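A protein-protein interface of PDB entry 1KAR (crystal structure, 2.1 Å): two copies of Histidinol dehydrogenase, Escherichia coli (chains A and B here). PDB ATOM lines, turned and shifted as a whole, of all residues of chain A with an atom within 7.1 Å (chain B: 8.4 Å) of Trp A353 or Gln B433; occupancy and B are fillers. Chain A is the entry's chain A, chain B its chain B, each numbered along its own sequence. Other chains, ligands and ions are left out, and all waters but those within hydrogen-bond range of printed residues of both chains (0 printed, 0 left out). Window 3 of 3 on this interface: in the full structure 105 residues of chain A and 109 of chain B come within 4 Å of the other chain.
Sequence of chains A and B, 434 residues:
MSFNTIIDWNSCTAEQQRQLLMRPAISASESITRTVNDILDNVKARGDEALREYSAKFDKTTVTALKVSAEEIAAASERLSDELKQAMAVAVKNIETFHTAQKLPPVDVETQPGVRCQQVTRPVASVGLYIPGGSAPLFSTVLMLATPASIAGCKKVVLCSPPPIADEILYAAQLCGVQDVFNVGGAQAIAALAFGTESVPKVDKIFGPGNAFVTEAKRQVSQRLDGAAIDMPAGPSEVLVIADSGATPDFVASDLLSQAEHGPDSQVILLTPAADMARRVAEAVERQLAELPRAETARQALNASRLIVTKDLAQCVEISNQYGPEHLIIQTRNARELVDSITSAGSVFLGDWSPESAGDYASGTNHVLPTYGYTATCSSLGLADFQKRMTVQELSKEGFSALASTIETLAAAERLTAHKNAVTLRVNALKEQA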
ATOM      1  N   THR A 248      37.577  -4.088  -3.420  1.00  0.00           N
ATOM      2  CA  THR A 248      37.183  -5.492  -3.373  1.00  0.00           C
ATOM      3  C   THR A 248      37.706  -6.221  -4.604  1.00  0.00           C
ATOM      4  O   THR A 248      37.236  -5.983  -5.718  1.00  0.00           O
ATOM      5  CB  THR A 248      35.654  -5.641  -3.340  1.00  0.00           C
ATOM      6  OG1 THR A 248      35.139  -4.985  -2.179  1.00  0.00           O
ATOM      7  CG2 THR A 248      35.261  -7.116  -3.305  1.00  0.00           C
ATOM      8  N   PHE A 251      35.352  -7.156  -7.371  1.00  0.00           N
ATOM      9  CA  PHE A 251      34.760  -6.031  -8.102  1.00  0.00           C
ATOM     10  C   PHE A 251      35.731  -5.532  -9.170  1.00  0.00           C
ATOM     11  O   PHE A 251      35.341  -5.246 -10.299  1.00  0.00           O
ATOM     12  CB  PHE A 251      34.439  -4.860  -7.163  1.00  0.00           C
ATOM     13  CG  PHE A 251      33.295  -5.107  -6.217  1.00  0.00           C
ATOM     14  CD1 PHE A 251      32.613  -6.321  -6.205  1.00  0.00           C
ATOM     15  CD2 PHE A 251      32.927  -4.122  -5.301  1.00  0.00           C
ATOM     16  CE1 PHE A 251      31.586  -6.557  -5.292  1.00  0.00           C
ATOM     17  CE2 PHE A 251      31.899  -4.349  -4.381  1.00  0.00           C
ATOM     18  CZ  PHE A 251      31.228  -5.572  -4.377  1.00  0.00           C
ATOM     19  N   GLN A 331      38.390   2.781  -7.930  1.00  0.00           N
ATOM     20  CA  GLN A 331      37.855   2.051  -6.795  1.00  0.00           C
ATOM     21  C   GLN A 331      38.732   2.299  -5.566  1.00  0.00           C
ATOM     22  O   GLN A 331      39.410   1.405  -5.079  1.00  0.00           O
ATOM     23  CB  GLN A 331      37.745   0.558  -7.136  1.00  0.00           C
ATOM     24  CG  GLN A 331      36.512   0.234  -7.980  1.00  0.00           C
ATOM     25  CD  GLN A 331      36.481  -1.199  -8.480  1.00  0.00           C
ATOM     26  OE1 GLN A 331      36.764  -2.139  -7.737  1.00  0.00           O
ATOM     27  NE2 GLN A 331      36.123  -1.374  -9.745  1.00  0.00           N
ATOM     28  N   ARG A 333      38.943   4.762  -1.671  1.00  0.00           N
ATOM     29  CA  ARG A 333      38.039   5.232  -0.628  1.00  0.00           C
ATOM     30  C   ARG A 333      37.592   6.696  -0.709  1.00  0.00           C
ATOM     31  O   ARG A 333      36.581   7.079  -0.112  1.00  0.00           O
ATOM     32  CB  ARG A 333      38.640   4.931   0.749  1.00  0.00           C
ATOM     33  CG  ARG A 333      38.086   3.637   1.379  1.00  0.00           C
ATOM     34  CD  ARG A 333      38.693   2.345   0.825  1.00  0.00           C
ATOM     35  NE  ARG A 333      38.499   2.094  -0.608  1.00  0.00           N
ATOM     36  CZ  ARG A 333      37.372   1.672  -1.182  1.00  0.00           C
ATOM     37  NH1 ARG A 333      36.279   1.443  -0.463  1.00  0.00           N
ATOM     38  NH2 ARG A 333      37.351   1.439  -2.490  1.00  0.00           N
ATOM     39  N   LEU A 350      33.315   6.248 -10.508  1.00  0.00           N
ATOM     40  CA  LEU A 350      33.767   6.415  -9.131  1.00  0.00           C
ATOM     41  C   LEU A 350      33.176   5.447  -8.113  1.00  0.00           C
ATOM     42  O   LEU A 350      31.985   5.165  -8.136  1.00  0.00           O
ATOM     43  CB  LEU A 350      33.472   7.849  -8.677  1.00  0.00           C
ATOM     44  CG  LEU A 350      33.986   8.985  -9.571  1.00  0.00           C
ATOM     45  CD1 LEU A 350      33.455  10.307  -9.070  1.00  0.00           C
ATOM     46  CD2 LEU A 350      35.501   8.995  -9.579  1.00  0.00           C
ATOM     47  N   GLY A 351      34.023   4.950  -7.216  1.00  0.00           N
ATOM     48  CA  GLY A 351      33.564   4.047  -6.172  1.00  0.00           C
ATOM     49  C   GLY A 351      33.380   2.591  -6.560  1.00  0.00           C
ATOM     50  O   GLY A 351      33.565   2.214  -7.717  1.00  0.00           O
ATOM     51  N   ASP A 352      32.984   1.775  -5.585  1.00  0.00           N
ATOM     52  CA  ASP A 352      32.792   0.345  -5.794  1.00  0.00           C
ATOM     53  C   ASP A 352      31.462  -0.042  -6.407  1.00  0.00           C
ATOM     54  O   ASP A 352      31.256  -1.214  -6.740  1.00  0.00           O
ATOM     55  CB  ASP A 352      32.917  -0.414  -4.473  1.00  0.00           C
ATOM     56  CG  ASP A 352      34.211  -0.133  -3.752  1.00  0.00           C
ATOM     57  OD1 ASP A 352      35.268  -0.026  -4.413  1.00  0.00           O
ATOM     58  OD2 ASP A 352      34.168  -0.033  -2.507  1.00  0.00           O
ATOM     59  N   TRP A 353      30.552   0.913  -6.559  1.00  0.00           N
ATOM     60  CA  TRP A 353      29.242   0.576  -7.103  1.00  0.00           C
ATOM     61  C   TRP A 353      28.960   1.182  -8.462  1.00  0.00           C
ATOM     62  O   TRP A 353      27.805   1.257  -8.884  1.00  0.00           O
ATOM     63  CB  TRP A 353      28.155   0.969  -6.098  1.00  0.00           C
ATOM     64  CG  TRP A 353      28.594   0.660  -4.709  1.00  0.00           C
ATOM     65  CD1 TRP A 353      29.187   1.520  -3.827  1.00  0.00           C
ATOM     66  CD2 TRP A 353      28.646  -0.634  -4.101  1.00  0.00           C
ATOM     67  NE1 TRP A 353      29.613   0.837  -2.715  1.00  0.00           N
ATOM     68  CE2 TRP A 353      29.292  -0.487  -2.858  1.00  0.00           C
ATOM     69  CE3 TRP A 353      28.212  -1.905  -4.490  1.00  0.00           C
ATOM     70  CZ2 TRP A 353      29.519  -1.564  -2.000  1.00  0.00           C
ATOM     71  CZ3 TRP A 353      28.438  -2.974  -3.640  1.00  0.00           C
ATOM     72  CH2 TRP A 353      29.085  -2.797  -2.409  1.00  0.00           C
ATOM     73  N   SER A 354      30.024   1.607  -9.147  1.00  0.00           N
ATOM     74  CA  SER A 354      29.894   2.189 -10.479  1.00  0.00           C
ATOM     75  C   SER A 354      30.594   1.286 -11.497  1.00  0.00           C
ATOM     76  O   SER A 354      31.598   1.659 -12.095  1.00  0.00           O
ATOM     77  CB  SER A 354      30.511   3.591 -10.501  1.00  0.00           C
ATOM     78  OG  SER A 354      29.946   4.405  -9.474  1.00  0.00           O
ATOM     79  N   PRO A 355      30.075   0.073 -11.697  1.00  0.00           N
ATOM     80  CA  PRO A 355      30.716  -0.822 -12.662  1.00  0.00           C
ATOM     81  C   PRO A 355      30.694  -0.251 -14.074  1.00  0.00           C
ATOM     82  O   PRO A 355      29.815   0.541 -14.423  1.00  0.00           O
ATOM     83  CB  PRO A 355      29.898  -2.107 -12.539  1.00  0.00           C
ATOM     84  CG  PRO A 355      28.535  -1.597 -12.150  1.00  0.00           C
ATOM     85  CD  PRO A 355      28.877  -0.556 -11.113  1.00  0.00           C
ATOM     86  N   ALA A 358      27.548  -0.342 -15.871  1.00  0.00           N
ATOM     87  CA  ALA A 358      26.519   0.620 -15.509  1.00  0.00           C
ATOM     88  C   ALA A 358      26.550   1.746 -16.538  1.00  0.00           C
ATOM     89  O   ALA A 358      25.509   2.182 -17.023  1.00  0.00           O
ATOM     90  CB  ALA A 358      26.779   1.182 -14.110  1.00  0.00           C
ATOM     91  N   GLY B 114      20.691   8.677  -6.602  1.00  0.00           N
ATOM     92  CA  GLY B 114      21.917   7.923  -6.427  1.00  0.00           C
ATOM     93  C   GLY B 114      22.751   7.670  -7.672  1.00  0.00           C
ATOM     94  O   GLY B 114      23.805   7.038  -7.584  1.00  0.00           O
ATOM     95  N   VAL B 115      22.287   8.131  -8.831  1.00  0.00           N
ATOM     96  CA  VAL B 115      23.052   7.955 -10.063  1.00  0.00           C
ATOM     97  C   VAL B 115      23.463   9.337 -10.568  1.00  0.00           C
ATOM     98  O   VAL B 115      22.755   9.961 -11.353  1.00  0.00           O
ATOM     99  CB  VAL B 115      22.234   7.226 -11.150  1.00  0.00           C
ATOM    100  CG1 VAL B 115      23.085   7.063 -12.407  1.00  0.00           C
ATOM    101  CG2 VAL B 115      21.781   5.846 -10.636  1.00  0.00           C
ATOM    102  N   GLN B 393      30.807   9.582 -13.594  1.00  0.00           N
ATOM    103  CA  GLN B 393      29.600   9.056 -12.969  1.00  0.00           C
ATOM    104  C   GLN B 393      29.922   8.321 -11.692  1.00  0.00           C
ATOM    105  O   GLN B 393      30.989   7.707 -11.560  1.00  0.00           O
ATOM    106  CB  GLN B 393      28.846   8.114 -13.908  1.00  0.00           C
ATOM    107  CG  GLN B 393      29.659   6.937 -14.396  1.00  0.00           C
ATOM    108  CD  GLN B 393      28.868   6.051 -15.327  1.00  0.00           C
ATOM    109  OE1 GLN B 393      28.165   5.146 -14.885  1.00  0.00           O
ATOM    110  NE2 GLN B 393      28.963   6.316 -16.619  1.00  0.00           N
ATOM    111  N   GLU B 394      28.990   8.394 -10.751  1.00  0.00           N
ATOM    112  CA  GLU B 394      29.121   7.722  -9.468  1.00  0.00           C
ATOM    113  C   GLU B 394      27.739   7.302  -8.989  1.00  0.00           C
ATOM    114  O   GLU B 394      26.846   8.135  -8.817  1.00  0.00           O
ATOM    115  CB  GLU B 394      29.771   8.644  -8.430  1.00  0.00           C
ATOM    116  CG  GLU B 394      29.769   8.076  -7.020  1.00  0.00           C
ATOM    117  CD  GLU B 394      30.538   8.939  -6.036  1.00  0.00           C
ATOM    118  OE1 GLU B 394      30.516  10.179  -6.181  1.00  0.00           O
ATOM    119  OE2 GLU B 394      31.157   8.377  -5.108  1.00  0.00           O
ATOM    120  N   LEU B 395      27.559   6.005  -8.795  1.00  0.00           N
ATOM    121  CA  LEU B 395      26.284   5.497  -8.325  1.00  0.00           C
ATOM    122  C   LEU B 395      26.445   5.136  -6.855  1.00  0.00           C
ATOM    123  O   LEU B 395      27.444   4.539  -6.473  1.00  0.00           O
ATOM    124  CB  LEU B 395      25.868   4.257  -9.122  1.00  0.00           C
ATOM    125  CG  LEU B 395      25.601   4.380 -10.633  1.00  0.00           C
ATOM    126  CD1 LEU B 395      26.884   4.732 -11.377  1.00  0.00           C
ATOM    127  CD2 LEU B 395      25.049   3.056 -11.151  1.00  0.00           C
ATOM    128  N   SER B 396      25.491   5.524  -6.023  1.00  0.00           N
ATOM    129  CA  SER B 396      25.565   5.177  -4.611  1.00  0.00           C
ATOM    130  C   SER B 396      25.083   3.735  -4.543  1.00  0.00           C
ATOM    131  O   SER B 396      24.647   3.179  -5.552  1.00  0.00           O
ATOM    132  CB  SER B 396      24.627   6.056  -3.791  1.00  0.00           C
ATOM    133  OG  SER B 396      23.285   5.806  -4.171  1.00  0.00           O
ATOM    134  N   LYS B 397      25.154   3.124  -3.367  1.00  0.00           N
ATOM    135  CA  LYS B 397      24.689   1.744  -3.218  1.00  0.00           C
ATOM    136  C   LYS B 397      23.209   1.713  -3.585  1.00  0.00           C
ATOM    137  O   LYS B 397      22.732   0.810  -4.280  1.00  0.00           O
ATOM    138  CB  LYS B 397      24.865   1.273  -1.777  1.00  0.00           C
ATOM    139  CG  LYS B 397      26.271   1.415  -1.240  1.00  0.00           C
ATOM    140  CD  LYS B 397      26.354   0.893   0.179  1.00  0.00           C
ATOM    141  CE  LYS B 397      27.786   0.887   0.677  1.00  0.00           C
ATOM    142  NZ  LYS B 397      27.840   0.376   2.074  1.00  0.00           N
ATOM    143  N   GLU B 398      22.481   2.716  -3.106  1.00  0.00           N
ATOM    144  CA  GLU B 398      21.059   2.824  -3.388  1.00  0.00           C
ATOM    145  C   GLU B 398      20.853   2.981  -4.893  1.00  0.00           C
ATOM    146  O   GLU B 398      20.043   2.279  -5.487  1.00  0.00           O
ATOM    147  CB  GLU B 398      20.460   4.031  -2.655  1.00  0.00           C
ATOM    148  CG  GLU B 398      20.455   3.939  -1.124  1.00  0.00           C
ATOM    149  CD  GLU B 398      21.853   3.860  -0.516  1.00  0.00           C
ATOM    150  OE1 GLU B 398      22.737   4.644  -0.937  1.00  0.00           O
ATOM    151  OE2 GLU B 398      22.062   3.022   0.395  1.00  0.00           O
ATOM    152  N   GLY B 399      21.593   3.905  -5.501  1.00  0.00           N
ATOM    153  CA  GLY B 399      21.469   4.142  -6.932  1.00  0.00           C
ATOM    154  C   GLY B 399      21.815   2.912  -7.738  1.00  0.00           C
ATOM    155  O   GLY B 399      21.108   2.550  -8.674  1.00  0.00           O
ATOM    156  N   PHE B 400      22.912   2.258  -7.375  1.00  0.00           N
ATOM    157  CA  PHE B 400      23.317   1.049  -8.074  1.00  0.00           C
ATOM    158  C   PHE B 400      22.259  -0.038  -7.905  1.00  0.00           C
ATOM    159  O   PHE B 400      21.877  -0.719  -8.864  1.00  0.00           O
ATOM    160  CB  PHE B 400      24.657   0.542  -7.533  1.00  0.00           C
ATOM    161  CG  PHE B 400      24.947  -0.881  -7.904  1.00  0.00           C
ATOM    162  CD1 PHE B 400      24.521  -1.923  -7.090  1.00  0.00           C
ATOM    163  CD2 PHE B 400      25.559  -1.183  -9.115  1.00  0.00           C
ATOM    164  CE1 PHE B 400      24.693  -3.243  -7.483  1.00  0.00           C
ATOM    165  CE2 PHE B 400      25.736  -2.497  -9.519  1.00  0.00           C
ATOM    166  CZ  PHE B 400      25.302  -3.531  -8.707  1.00  0.00           C
ATOM    167  N   SER B 401      21.784  -0.196  -6.675  1.00  0.00           N
ATOM    168  CA  SER B 401      20.786  -1.216  -6.380  1.00  0.00           C
ATOM    169  C   SER B 401      19.494  -1.010  -7.154  1.00  0.00           C
ATOM    170  O   SER B 401      18.860  -1.977  -7.582  1.00  0.00           O
ATOM    171  CB  SER B 401      20.490  -1.252  -4.879  1.00  0.00           C
ATOM    172  OG  SER B 401      21.634  -1.656  -4.148  1.00  0.00           O
ATOM    173  N   LEU B 403      19.238   0.304 -10.067  1.00  0.00           N
ATOM    174  CA  LEU B 403      19.491   0.162 -11.498  1.00  0.00           C
ATOM    175  C   LEU B 403      20.032  -1.205 -11.909  1.00  0.00           C
ATOM    176  O   LEU B 403      20.173  -1.485 -13.098  1.00  0.00           O
ATOM    177  CB  LEU B 403      20.472   1.257 -11.927  1.00  0.00           C
ATOM    178  CG  LEU B 403      20.425   1.851 -13.333  1.00  0.00           C
ATOM    179  CD1 LEU B 403      19.047   2.435 -13.589  1.00  0.00           C
ATOM    180  CD2 LEU B 403      21.500   2.936 -13.464  1.00  0.00           C
ATOM    181  N   ILE B 407      20.466  -3.251 -15.782  1.00  0.00           N
ATOM    182  CA  ILE B 407      21.782  -3.532 -16.336  1.00  0.00           C
ATOM    183  C   ILE B 407      21.935  -5.002 -16.683  1.00  0.00           C
ATOM    184  O   ILE B 407      22.375  -5.338 -17.786  1.00  0.00           O
ATOM    185  CB  ILE B 407      22.895  -3.119 -15.359  1.00  0.00           C
ATOM    186  CG1 ILE B 407      22.731  -1.645 -14.992  1.00  0.00           C
ATOM    187  CG2 ILE B 407      24.273  -3.339 -16.006  1.00  0.00           C
ATOM    188  CD1 ILE B 407      23.595  -1.212 -13.833  1.00  0.00           C
ATOM    189  N   ALA B 422      29.448  -8.507 -13.286  1.00  0.00           N
ATOM    190  CA  ALA B 422      29.968  -7.385 -12.524  1.00  0.00           C
ATOM    191  C   ALA B 422      28.842  -6.780 -11.688  1.00  0.00           C
ATOM    192  O   ALA B 422      29.098  -6.153 -10.660  1.00  0.00           O
ATOM    193  CB  ALA B 422      30.570  -6.331 -13.464  1.00  0.00           C
ATOM    194  N   VAL B 423      27.598  -6.978 -12.123  1.00  0.00           N
ATOM    195  CA  VAL B 423      26.443  -6.459 -11.386  1.00  0.00           C
ATOM    196  C   VAL B 423      26.079  -7.451 -10.283  1.00  0.00           C
ATOM    197  O   VAL B 423      25.982  -7.078  -9.112  1.00  0.00           O
ATOM    198  CB  VAL B 423      25.204  -6.256 -12.308  1.00  0.00           C
ATOM    199  CG1 VAL B 423      24.001  -5.732 -11.487  1.00  0.00           C
ATOM    200  CG2 VAL B 423      25.533  -5.255 -13.409  1.00  0.00           C
ATOM    201  N   THR B 424      25.897  -8.715 -10.658  1.00  0.00           N
ATOM    202  CA  THR B 424      25.533  -9.758  -9.701  1.00  0.00           C
ATOM    203  C   THR B 424      26.440  -9.770  -8.464  1.00  0.00           C
ATOM    204  O   THR B 424      25.954  -9.838  -7.333  1.00  0.00           O
ATOM    205  CB  THR B 424      25.586 -11.144 -10.358  1.00  0.00           C
ATOM    206  OG1 THR B 424      24.800 -11.134 -11.557  1.00  0.00           O
ATOM    207  CG2 THR B 424      25.028 -12.204  -9.412  1.00  0.00           C
ATOM    208  N   LEU B 425      27.750  -9.694  -8.685  1.00  0.00           N
ATOM    209  CA  LEU B 425      28.723  -9.707  -7.594  1.00  0.00           C
ATOM    210  C   LEU B 425      28.451  -8.595  -6.592  1.00  0.00           C
ATOM    211  O   LEU B 425      28.466  -8.808  -5.376  1.00  0.00           O
ATOM    212  CB  LEU B 425      30.146  -9.549  -8.149  1.00  0.00           C
ATOM    213  CG  LEU B 425      30.804 -10.750  -8.822  1.00  0.00           C
ATOM    214  CD1 LEU B 425      32.104 -10.319  -9.464  1.00  0.00           C
ATOM    215  CD2 LEU B 425      31.059 -11.842  -7.787  1.00  0.00           C
ATOM    216  N   ARG B 426      28.205  -7.399  -7.115  1.00  0.00           N
ATOM    217  CA  ARG B 426      27.925  -6.250  -6.280  1.00  0.00           C
ATOM    218  C   ARG B 426      26.598  -6.428  -5.539  1.00  0.00           C
ATOM    219  O   ARG B 426      26.522  -6.179  -4.336  1.00  0.00           O
ATOM    220  CB  ARG B 426      27.924  -4.986  -7.144  1.00  0.00           C
ATOM    221  CG  ARG B 426      29.322  -4.634  -7.689  1.00  0.00           C
ATOM    222  CD  ARG B 426      29.253  -3.482  -8.681  1.00  0.00           C
ATOM    223  NE  ARG B 426      30.551  -2.851  -8.905  1.00  0.00           N
ATOM    224  CZ  ARG B 426      31.549  -3.382  -9.604  1.00  0.00           C
ATOM    225  NH1 ARG B 426      31.419  -4.571 -10.164  1.00  0.00           N
ATOM    226  NH2 ARG B 426      32.679  -2.704  -9.759  1.00  0.00           N
ATOM    227  N   VAL B 427      25.565  -6.876  -6.249  1.00  0.00           N
ATOM    228  CA  VAL B 427      24.256  -7.092  -5.639  1.00  0.00           C
ATOM    229  C   VAL B 427      24.374  -8.085  -4.483  1.00  0.00           C
ATOM    230  O   VAL B 427      23.815  -7.858  -3.410  1.00  0.00           O
ATOM    231  CB  VAL B 427      23.219  -7.624  -6.676  1.00  0.00           C
ATOM    232  CG1 VAL B 427      21.928  -8.053  -5.971  1.00  0.00           C
ATOM    233  CG2 VAL B 427      22.886  -6.529  -7.685  1.00  0.00           C
ATOM    234  N   ASN B 428      25.116  -9.172  -4.688  1.00  0.00           N
ATOM    235  CA  ASN B 428      25.269 -10.166  -3.636  1.00  0.00           C
ATOM    236  C   ASN B 428      26.069  -9.635  -2.454  1.00  0.00           C
ATOM    237  O   ASN B 428      25.764  -9.947  -1.303  1.00  0.00           O
ATOM    238  CB  ASN B 428      25.912 -11.446  -4.178  1.00  0.00           C
ATOM    239  CG  ASN B 428      24.975 -12.217  -5.083  1.00  0.00           C
ATOM    240  OD1 ASN B 428      23.763 -12.100  -4.960  1.00  0.00           O
ATOM    241  ND2 ASN B 428      25.530 -13.014  -5.987  1.00  0.00           N
ATOM    242  N   ALA B 429      27.089  -8.831  -2.737  1.00  0.00           N
ATOM    243  CA  ALA B 429      27.906  -8.253  -1.679  1.00  0.00           C
ATOM    244  C   ALA B 429      27.032  -7.350  -0.795  1.00  0.00           C
ATOM    245  O   ALA B 429      27.223  -7.286   0.423  1.00  0.00           O
ATOM    246  CB  ALA B 429      29.061  -7.449  -2.285  1.00  0.00           C
ATOM    247  N   LEU B 430      26.074  -6.655  -1.410  1.00  0.00           N
ATOM    248  CA  LEU B 430      25.186  -5.774  -0.655  1.00  0.00           C
ATOM    249  C   LEU B 430      24.180  -6.564   0.193  1.00  0.00           C
ATOM    250  O   LEU B 430      23.852  -6.157   1.311  1.00  0.00           O
ATOM    251  CB  LEU B 430      24.466  -4.802  -1.596  1.00  0.00           C
ATOM    252  CG  LEU B 430      25.348  -3.682  -2.172  1.00  0.00           C
ATOM    253  CD1 LEU B 430      24.534  -2.843  -3.125  1.00  0.00           C
ATOM    254  CD2 LEU B 430      25.908  -2.811  -1.050  1.00  0.00           C
ATOM    255  N   LYS B 431      23.687  -7.686  -0.330  1.00  0.00           N
ATOM    256  CA  LYS B 431      22.765  -8.524   0.441  1.00  0.00           C
ATOM    257  C   LYS B 431      23.536  -8.956   1.691  1.00  0.00           C
ATOM    258  O   LYS B 431      23.128  -8.690   2.824  1.00  0.00           O
ATOM    259  CB  LYS B 431      22.379  -9.791  -0.325  1.00  0.00           C
ATOM    260  CG  LYS B 431      21.602  -9.595  -1.608  1.00  0.00           C
ATOM    261  CD  LYS B 431      21.262 -10.958  -2.214  1.00  0.00           C
ATOM    262  CE  LYS B 431      20.291 -10.828  -3.374  1.00  0.00           C
ATOM    263  NZ  LYS B 431      19.911 -12.160  -3.905  1.00  0.00           N
ATOM    264  N   GLU B 432      24.660  -9.630   1.459  1.00  0.00           N
ATOM    265  CA  GLU B 432      25.515 -10.114   2.533  1.00  0.00           C
ATOM    266  C   GLU B 432      25.667  -9.040   3.606  1.00  0.00           C
ATOM    267  O   GLU B 432      25.365  -9.275   4.776  1.00  0.00           O
ATOM    268  CB  GLU B 432      26.883 -10.507   1.965  1.00  0.00           C
ATOM    269  CG  GLU B 432      27.840 -11.152   2.960  1.00  0.00           C
ATOM    270  CD  GLU B 432      28.612 -10.143   3.796  1.00  0.00           C
ATOM    271  OE1 GLU B 432      29.449 -10.571   4.617  1.00  0.00           O
ATOM    272  OE2 GLU B 432      28.391  -8.925   3.632  1.00  0.00           O
ATOM    273  N   GLN B 433      26.118  -7.857   3.196  1.00  0.00           N
ATOM    274  CA  GLN B 433      26.311  -6.743   4.118  1.00  0.00           C
ATOM    275  C   GLN B 433      25.058  -6.435   4.934  1.00  0.00           C
ATOM    276  O   GLN B 433      25.130  -6.255   6.149  1.00  0.00           O
ATOM    277  CB  GLN B 433      26.742  -5.491   3.350  1.00  0.00           C
ATOM    278  CG  GLN B 433      28.225  -5.448   3.019  1.00  0.00           C
ATOM    279  CD  GLN B 433      28.598  -4.264   2.144  1.00  0.00           C
ATOM    280  OE1 GLN B 433      28.103  -3.151   2.341  1.00  0.00           O
ATOM    281  NE2 GLN B 433      29.486  -4.495   1.178  1.00  0.00           N
ATOM    282  N   ALA B 434      23.912  -6.375   4.259  1.00  0.00           N
ATOM    283  CA  ALA B 434      22.642  -6.082   4.915  1.00  0.00           C
ATOM    284  C   ALA B 434      21.462  -6.504   4.039  1.00  0.00           C
ATOM    285  O   ALA B 434      20.876  -5.622   3.372  1.00  0.00           O
ATOM    286  CB  ALA B 434      22.552  -4.587   5.240  1.00  0.00           C
ATOM    287  OXT ALA B 434      21.146  -7.716   4.019  1.00  0.00           O
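CZ of Phe A251 touches CB of Ala B429, at 3.5 Å. Leu A350 touches Glu B394. Trp A353 touches Leu B395. CG of Lys B397 touches NE1 of Trp A353, 3.7 Å away. Trp A353 touches Arg B426. Leu B430 touches Trp A353. NE2 of Gln B433 touches CH2 of Trp A353 (3.99 Å). CD of Pro A355 touches CD2 of Phe B400, 3.9 Å away. Pro A355 touches Arg B426. Ala A358 touches Ile B407.
Printed residues of chain A that touch a printed residue of chain B: Phe A251, Gln A331, Leu A350, Asp A352, Trp A353, Ser A354, Pro A355 and Ala A358. Among the printed residues, 19 pairs touch across the chains.
No position is printed for both chains.
Of the printed residues of chain B, Leu A350 touches Gln B393 (2.9 Å) and Glu B394 (3.8 Å). Printed residues of chain B within 4 Å of Trp A353: Leu B395, Lys B397, Phe B400, Arg B426, Leu B430 and Gln B433. Of the printed residues of chain B, Pro A355 touches Phe B400 (3.9 Å) and Arg B426 (3.6 Å). Of the printed residues of chain A, Gln B393 touches Leu A350 (2.9 Å). Gly B399 touches none of the printed residues of chain A. Val B423 touches none of the printed residues of chain A. Of the printed residues of chain A, Ala B429 touches Phe A251 (3.5 Å). Of the printed residues of chain A, Gln B433 touches Trp A353. The nearest printed residue of chain B that does not touch Leu A350 is Leu B395 (4.6 Å).
The backbone carbonyl oxygen (O) of Gln A331 is in hydrogen-bond range of the guanidinium group (NH2) of Arg A333 (3.3 Å). The guanidinium group of Arg A333 is in salt-bridge range of the side-chain carboxylate of Asp A352, 3.2 Å away. OG of Ser A354 is in hydrogen-bond range of O of Leu A350 (2.6 Å). The backbone carbonyl oxygen of Lys B397 is in hydrogen-bond range of the side-chain hydroxyl of Ser B401 (2.7 Å). O of Ala B422 lies within hydrogen-bond range of NH1 of Arg B426, at 2.9 Å.
N of Leu A350 is in hydrogen-bond range of O of Gln B393 (2.9 Å). O of Asp A352 sits at hydrogen-bond distance from NE of Arg B426 (2.8 Å). N of Leu B395 sits at hydrogen-bond distance from OG of Ser A354, 3.0 Å away.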
